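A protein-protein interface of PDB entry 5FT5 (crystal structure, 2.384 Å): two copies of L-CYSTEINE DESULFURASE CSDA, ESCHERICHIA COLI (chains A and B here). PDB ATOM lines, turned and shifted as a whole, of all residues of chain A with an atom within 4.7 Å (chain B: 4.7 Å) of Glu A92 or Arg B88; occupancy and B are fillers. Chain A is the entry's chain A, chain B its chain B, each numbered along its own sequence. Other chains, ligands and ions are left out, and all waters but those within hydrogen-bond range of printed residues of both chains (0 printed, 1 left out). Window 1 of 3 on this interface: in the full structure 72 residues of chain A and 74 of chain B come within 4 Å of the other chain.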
ATOM      1  N   TRP A  86      28.391   6.948 -28.705  1.00  0.00           N
ATOM      2  CA  TRP A  86      28.071   5.554 -29.030  1.00  0.00           C
ATOM      3  C   TRP A  86      28.492   4.609 -27.911  1.00  0.00           C
ATOM      4  O   TRP A  86      29.570   4.757 -27.339  1.00  0.00           O
ATOM      5  CB  TRP A  86      28.730   5.116 -30.350  1.00  0.00           C
ATOM      6  CG  TRP A  86      28.373   5.976 -31.522  1.00  0.00           C
ATOM      7  CD1 TRP A  86      29.229   6.706 -32.290  1.00  0.00           C
ATOM      8  CD2 TRP A  86      27.060   6.213 -32.047  1.00  0.00           C
ATOM      9  NE1 TRP A  86      28.534   7.377 -33.268  1.00  0.00           N
ATOM     10  CE2 TRP A  86      27.200   7.096 -33.136  1.00  0.00           C
ATOM     11  CE3 TRP A  86      25.781   5.766 -31.701  1.00  0.00           C
ATOM     12  CZ2 TRP A  86      26.109   7.535 -33.886  1.00  0.00           C
ATOM     13  CZ3 TRP A  86      24.696   6.208 -32.446  1.00  0.00           C
ATOM     14  CH2 TRP A  86      24.870   7.080 -33.526  1.00  0.00           C
ATOM     15  N   THR A  87      27.630   3.646 -27.600  1.00  0.00           N
ATOM     16  CA  THR A  87      27.943   2.591 -26.640  1.00  0.00           C
ATOM     17  C   THR A  87      27.406   1.273 -27.188  1.00  0.00           C
ATOM     18  O   THR A  87      26.898   1.228 -28.306  1.00  0.00           O
ATOM     19  CB  THR A  87      27.321   2.867 -25.244  1.00  0.00           C
ATOM     20  OG1 THR A  87      25.891   2.788 -25.320  1.00  0.00           O
ATOM     21  CG2 THR A  87      27.724   4.240 -24.736  1.00  0.00           C
ATOM     22  N   ARG A  88      27.522   0.206 -26.405  1.00  0.00           N
ATOM     23  CA  ARG A  88      27.025  -1.096 -26.830  1.00  0.00           C
ATOM     24  C   ARG A  88      25.638  -1.388 -26.268  1.00  0.00           C
ATOM     25  O   ARG A  88      25.085  -2.464 -26.489  1.00  0.00           O
ATOM     26  CB  ARG A  88      28.005  -2.211 -26.452  1.00  0.00           C
ATOM     27  CG  ARG A  88      28.746  -1.962 -25.156  1.00  0.00           C
ATOM     28  CD  ARG A  88      28.858  -3.228 -24.327  1.00  0.00           C
ATOM     29  NE  ARG A  88      29.755  -4.213 -24.921  1.00  0.00           N
ATOM     30  CZ  ARG A  88      30.023  -5.395 -24.375  1.00  0.00           C
ATOM     31  NH1 ARG A  88      29.459  -5.736 -23.224  1.00  0.00           N
ATOM     32  NH2 ARG A  88      30.852  -6.234 -24.976  1.00  0.00           N
ATOM     33  N   GLY A  89      25.079  -0.422 -25.544  1.00  0.00           N
ATOM     34  CA  GLY A  89      23.739  -0.555 -24.999  1.00  0.00           C
ATOM     35  C   GLY A  89      23.455   0.409 -23.860  1.00  0.00           C
ATOM     36  O   GLY A  89      24.356   1.091 -23.372  1.00  0.00           O
ATOM     37  N   THR A  90      22.194   0.464 -23.440  1.00  0.00           N
ATOM     38  CA  THR A  90      21.795   1.273 -22.292  1.00  0.00           C
ATOM     39  C   THR A  90      22.669   0.986 -21.079  1.00  0.00           C
ATOM     40  O   THR A  90      23.029   1.896 -20.329  1.00  0.00           O
ATOM     41  CB  THR A  90      20.320   1.020 -21.903  1.00  0.00           C
ATOM     42  OG1 THR A  90      19.468   1.359 -23.003  1.00  0.00           O
ATOM     43  CG2 THR A  90      19.933   1.855 -20.679  1.00  0.00           C
ATOM     44  N   THR A  91      23.005  -0.285 -20.894  1.00  0.00           N
ATOM     45  CA  THR A  91      23.783  -0.717 -19.739  1.00  0.00           C
ATOM     46  C   THR A  91      25.177  -0.090 -19.730  1.00  0.00           C
ATOM     47  O   THR A  91      25.630   0.416 -18.703  1.00  0.00           O
ATOM     48  CB  THR A  91      23.903  -2.252 -19.680  1.00  0.00           C
ATOM     49  OG1 THR A  91      22.617  -2.846 -19.889  1.00  0.00           O
ATOM     50  CG2 THR A  91      24.440  -2.692 -18.334  1.00  0.00           C
ATOM     51  N   GLU A  92      25.859  -0.116 -20.870  1.00  0.00           N
ATOM     52  CA  GLU A  92      27.160   0.536 -20.945  1.00  0.00           C
ATOM     53  C   GLU A  92      27.037   2.040 -20.708  1.00  0.00           C
ATOM     54  O   GLU A  92      27.854   2.624 -20.008  1.00  0.00           O
ATOM     55  CB  GLU A  92      27.879   0.278 -22.275  1.00  0.00           C
ATOM     56  CG  GLU A  92      29.226   1.000 -22.321  1.00  0.00           C
ATOM     57  CD  GLU A  92      29.922   0.931 -23.664  1.00  0.00           C
ATOM     58  OE1 GLU A  92      29.237   0.784 -24.697  1.00  0.00           O
ATOM     59  OE2 GLU A  92      31.167   1.027 -23.683  1.00  0.00           O
ATOM     60  N   SER A  93      26.021   2.663 -21.296  1.00  0.00           N
ATOM     61  CA  SER A  93      25.817   4.102 -21.141  1.00  0.00           C
ATOM     62  C   SER A  93      25.780   4.511 -19.668  1.00  0.00           C
ATOM     63  O   SER A  93      26.453   5.454 -19.254  1.00  0.00           O
ATOM     64  CB  SER A  93      24.526   4.546 -21.840  1.00  0.00           C
ATOM     65  OG  SER A  93      24.582   4.300 -23.237  1.00  0.00           O
ATOM     66  N   ILE A  94      24.997   3.783 -18.881  1.00  0.00           N
ATOM     67  CA  ILE A  94      24.810   4.105 -17.471  1.00  0.00           C
ATOM     68  C   ILE A  94      26.069   3.823 -16.654  1.00  0.00           C
ATOM     69  O   ILE A  94      26.455   4.624 -15.803  1.00  0.00           O
ATOM     70  CB  ILE A  94      23.590   3.360 -16.895  1.00  0.00           C
ATOM     71  CG1 ILE A  94      22.304   3.892 -17.545  1.00  0.00           C
ATOM     72  CG2 ILE A  94      23.537   3.485 -15.379  1.00  0.00           C
ATOM     73  CD1 ILE A  94      21.058   3.092 -17.203  1.00  0.00           C
ATOM     74  N   ASN A  95      26.710   2.688 -16.916  1.00  0.00           N
ATOM     75  CA  ASN A  95      28.004   2.388 -16.301  1.00  0.00           C
ATOM     76  C   ASN A  95      29.021   3.497 -16.566  1.00  0.00           C
ATOM     77  O   ASN A  95      29.859   3.792 -15.713  1.00  0.00           O
ATOM     78  CB  ASN A  95      28.551   1.038 -16.789  1.00  0.00           C
ATOM     79  CG  ASN A  95      27.952  -0.149 -16.042  1.00  0.00           C
ATOM     80  OD1 ASN A  95      28.441  -0.541 -14.983  1.00  0.00           O
ATOM     81  ND2 ASN A  95      26.892  -0.731 -16.600  1.00  0.00           N
ATOM     82  N   MET A  96      28.938   4.112 -17.745  1.00  0.00           N
ATOM     83  CA  MET A  96      29.833   5.214 -18.097  1.00  0.00           C
ATOM     84  C   MET A  96      29.616   6.422 -17.192  1.00  0.00           C
ATOM     85  O   MET A  96      30.570   7.008 -16.676  1.00  0.00           O
ATOM     86  CB  MET A  96      29.652   5.628 -19.563  1.00  0.00           C
ATOM     87  CG  MET A  96      30.256   4.657 -20.575  1.00  0.00           C
ATOM     88  SD  MET A  96      30.028   5.198 -22.286  1.00  0.00           S
ATOM     89  CE  MET A  96      30.745   6.837 -22.197  1.00  0.00           C
ATOM     90  N   GLY A 228      24.090  -4.650 -30.120  1.00  0.00           N
ATOM     91  CA  GLY A 228      25.442  -4.171 -29.865  1.00  0.00           C
ATOM     92  C   GLY A 228      25.680  -2.696 -30.145  1.00  0.00           C
ATOM     93  O   GLY A 228      26.809  -2.268 -30.395  1.00  0.00           O
ATOM     94  N   TRP A 245      36.516   6.970 -20.832  1.00  0.00           N
ATOM     95  CA  TRP A 245      35.940   5.679 -20.475  1.00  0.00           C
ATOM     96  C   TRP A 245      37.000   4.594 -20.661  1.00  0.00           C
ATOM     97  O   TRP A 245      37.753   4.298 -19.736  1.00  0.00           O
ATOM     98  CB  TRP A 245      34.697   5.420 -21.328  1.00  0.00           C
ATOM     99  CG  TRP A 245      33.958   4.149 -21.035  1.00  0.00           C
ATOM    100  CD1 TRP A 245      33.251   3.399 -21.928  1.00  0.00           C
ATOM    101  CD2 TRP A 245      33.847   3.478 -19.772  1.00  0.00           C
ATOM    102  NE1 TRP A 245      32.704   2.307 -21.303  1.00  0.00           N
ATOM    103  CE2 TRP A 245      33.054   2.330 -19.980  1.00  0.00           C
ATOM    104  CE3 TRP A 245      34.340   3.732 -18.491  1.00  0.00           C
ATOM    105  CZ2 TRP A 245      32.745   1.440 -18.954  1.00  0.00           C
ATOM    106  CZ3 TRP A 245      34.030   2.848 -17.472  1.00  0.00           C
ATOM    107  CH2 TRP A 245      33.242   1.716 -17.710  1.00  0.00           C
ATOM    108  N   THR B  87      33.287  -9.525 -25.733  1.00  0.00           N
ATOM    109  CA  THR B  87      33.491  -8.100 -25.532  1.00  0.00           C
ATOM    110  C   THR B  87      33.087  -7.408 -26.825  1.00  0.00           C
ATOM    111  O   THR B  87      32.509  -8.040 -27.708  1.00  0.00           O
ATOM    112  CB  THR B  87      34.961  -7.788 -25.201  1.00  0.00           C
ATOM    113  OG1 THR B  87      35.787  -8.102 -26.328  1.00  0.00           O
ATOM    114  CG2 THR B  87      35.420  -8.613 -24.005  1.00  0.00           C
ATOM    115  N   ARG B  88      33.388  -6.119 -26.941  1.00  0.00           N
ATOM    116  CA  ARG B  88      33.064  -5.385 -28.158  1.00  0.00           C
ATOM    117  C   ARG B  88      34.289  -5.258 -29.066  1.00  0.00           C
ATOM    118  O   ARG B  88      34.215  -4.675 -30.149  1.00  0.00           O
ATOM    119  CB  ARG B  88      32.492  -4.003 -27.830  1.00  0.00           C
ATOM    120  CG  ARG B  88      33.520  -3.006 -27.335  1.00  0.00           C
ATOM    121  CD  ARG B  88      33.385  -1.669 -28.054  1.00  0.00           C
ATOM    122  NE  ARG B  88      32.674  -0.665 -27.264  1.00  0.00           N
ATOM    123  CZ  ARG B  88      31.441  -0.238 -27.521  1.00  0.00           C
ATOM    124  NH1 ARG B  88      30.765  -0.724 -28.555  1.00  0.00           N
ATOM    125  NH2 ARG B  88      30.884   0.680 -26.743  1.00  0.00           N
ATOM    126  N   GLY B  89      35.411  -5.812 -28.620  1.00  0.00           N
ATOM    127  CA  GLY B  89      36.641  -5.761 -29.386  1.00  0.00           C
ATOM    128  C   GLY B  89      37.867  -5.976 -28.526  1.00  0.00           C
ATOM    129  O   GLY B  89      37.761  -6.168 -27.313  1.00  0.00           O
ATOM    130  N   GLU B  92      38.295  -3.409 -25.592  1.00  0.00           N
ATOM    131  CA  GLU B  92      37.513  -3.633 -24.374  1.00  0.00           C
ATOM    132  C   GLU B  92      38.091  -4.775 -23.545  1.00  0.00           C
ATOM    133  O   GLU B  92      38.171  -4.679 -22.317  1.00  0.00           O
ATOM    134  CB  GLU B  92      36.022  -3.882 -24.656  1.00  0.00           C
ATOM    135  CG  GLU B  92      35.195  -3.866 -23.364  1.00  0.00           C
ATOM    136  CD  GLU B  92      33.710  -4.186 -23.531  1.00  0.00           C
ATOM    137  OE1 GLU B  92      33.255  -4.510 -24.650  1.00  0.00           O
ATOM    138  OE2 GLU B  92      32.991  -4.117 -22.511  1.00  0.00           O
ATOM    139  N   GLY B 228      32.068  -4.697 -33.937  1.00  0.00           N
ATOM    140  CA  GLY B 228      31.444  -4.649 -32.627  1.00  0.00           C
ATOM    141  C   GLY B 228      31.469  -5.949 -31.847  1.00  0.00           C
ATOM    142  O   GLY B 228      30.666  -6.156 -30.938  1.00  0.00           O
ATOM    143  N   ILE B 229      32.393  -6.834 -32.188  1.00  0.00           N
ATOM    144  CA  ILE B 229      32.511  -8.083 -31.452  1.00  0.00           C
ATOM    145  C   ILE B 229      33.978  -8.434 -31.197  1.00  0.00           C
ATOM    146  O   ILE B 229      34.828  -8.304 -32.078  1.00  0.00           O
ATOM    147  CB  ILE B 229      31.761  -9.244 -32.160  1.00  0.00           C
ATOM    148  CG1 ILE B 229      31.798 -10.514 -31.305  1.00  0.00           C
ATOM    149  CG2 ILE B 229      32.321  -9.486 -33.554  1.00  0.00           C
ATOM    150  CD1 ILE B 229      31.025 -10.395 -29.986  1.00  0.00           C
ATOM    151  N   GLY B 230      34.266  -8.855 -29.972  1.00  0.00           N
ATOM    152  CA  GLY B 230      35.623  -9.171 -29.580  1.00  0.00           C
ATOM    153  C   GLY B 230      35.671 -10.345 -28.631  1.00  0.00           C
ATOM    154  O   GLY B 230      34.639 -10.849 -28.191  1.00  0.00           O
ATOM    155  N   LEU B 246      31.013  -4.427 -16.118  1.00  0.00           N
ATOM    156  CA  LEU B 246      29.882  -3.512 -16.098  1.00  0.00           C
ATOM    157  C   LEU B 246      28.768  -4.138 -15.272  1.00  0.00           C
ATOM    158  O   LEU B 246      28.553  -5.348 -15.333  1.00  0.00           O
ATOM    159  CB  LEU B 246      29.397  -3.224 -17.520  1.00  0.00           C
ATOM    160  CG  LEU B 246      30.440  -2.623 -18.469  1.00  0.00           C
ATOM    161  CD1 LEU B 246      29.814  -2.223 -19.798  1.00  0.00           C
ATOM    162  CD2 LEU B 246      31.129  -1.433 -17.810  1.00  0.00           C
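N of Arg B88 lies close to NH2 of Arg A88, at 3.2 Å. The guanidinium group (NH2) of Arg A88 lies within salt-bridge range of the side-chain carboxylate (OE1) of Glu B92. OE1 of Glu A92 is in salt-bridge range of NH2 of Arg B88 (2.6 Å).
N of Arg A88 is in hydrogen-bond range of OE1 of Glu A92 (2.5 Å). The side-chain hydroxyl of Thr B87 sits at hydrogen-bond distance from the backbone carbonyl oxygen of Gly B89, at 2.9 Å. The side-chain hydroxyl (OG1) of Thr A87 is in hydrogen-bond range of the side-chain hydroxyl (OG) of Ser A93, at 2.9 Å. The backbone carbonyl oxygen of Thr A91 is in hydrogen-bond range of the side-chain amide nitrogen of Asn A95, 2.7 Å away. The backbone NH (N) of Arg B88 sits at hydrogen-bond distance from the side-chain carboxylate (OE1) of Glu B92 (2.8 Å). The backbone carbonyl oxygen (O) of Arg B88 lies within hydrogen-bond range of the backbone NH (N) of Ile B229, 3.5 Å away.
Arg B88 touches Thr A87. NH2 of Arg A88 touches C of Thr B87, 3.1 Å away. Leu B246 touches Glu A92. Leu B246 touches Asn A95. CD2 of Leu B246 touches CZ2 of Trp A245, 3.5 Å away.
Of the printed residues of chain B, Thr A87 touches Arg B88 (3.5 Å). Printed residues of chain B within 4 Å of Arg A88: Thr B87, Arg B88 and Glu B92. Of the printed residues of chain B, Glu A92 touches Arg B88 and Leu B246. Printed residues of chain B within 4 Å of Trp A245: Leu B246. Of the printed residues of chain A, Thr B87 touches Arg A88. Of the printed residues of chain A, Arg B88 touches Thr A87 (3.5 Å), Arg A88 (3.2 Å) and Glu A92 (2.6 Å). The nearest printed residue of chain B that does not touch Glu A92 is Glu B92 (5.6 Å).
Of the 8 printed residues of chain B, 4 touch a printed residue of chain A. Hydrophobic or aromatic side chains of chain A within 4 Å of the printed part of chain B: Trp A245. Among the printed residues, 8 pairs touch across the chains. Among the printed residues, Asp or Glu carboxylates within 4 Å of a Lys or Arg side-chain nitrogen of the other chain: Arg A88 with Glu B92 (3.0 Å) and Glu A92 with Arg B88 (2.6 Å).
Thr A87 touches Arg B88, and with the chains exchanged Arg A88 touches Thr B87. Arg B88 touches its own counterpart, Arg A88. Arg A88 touches Glu B92, and with the chains exchanged Glu A92 touches Arg B88. Positions printed for both chains: 87, 88, 89, 92 and 228. Of the 8 pairs that touch across the chains among the printed residues, 5 have their exchanged pair printed and touching as well.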
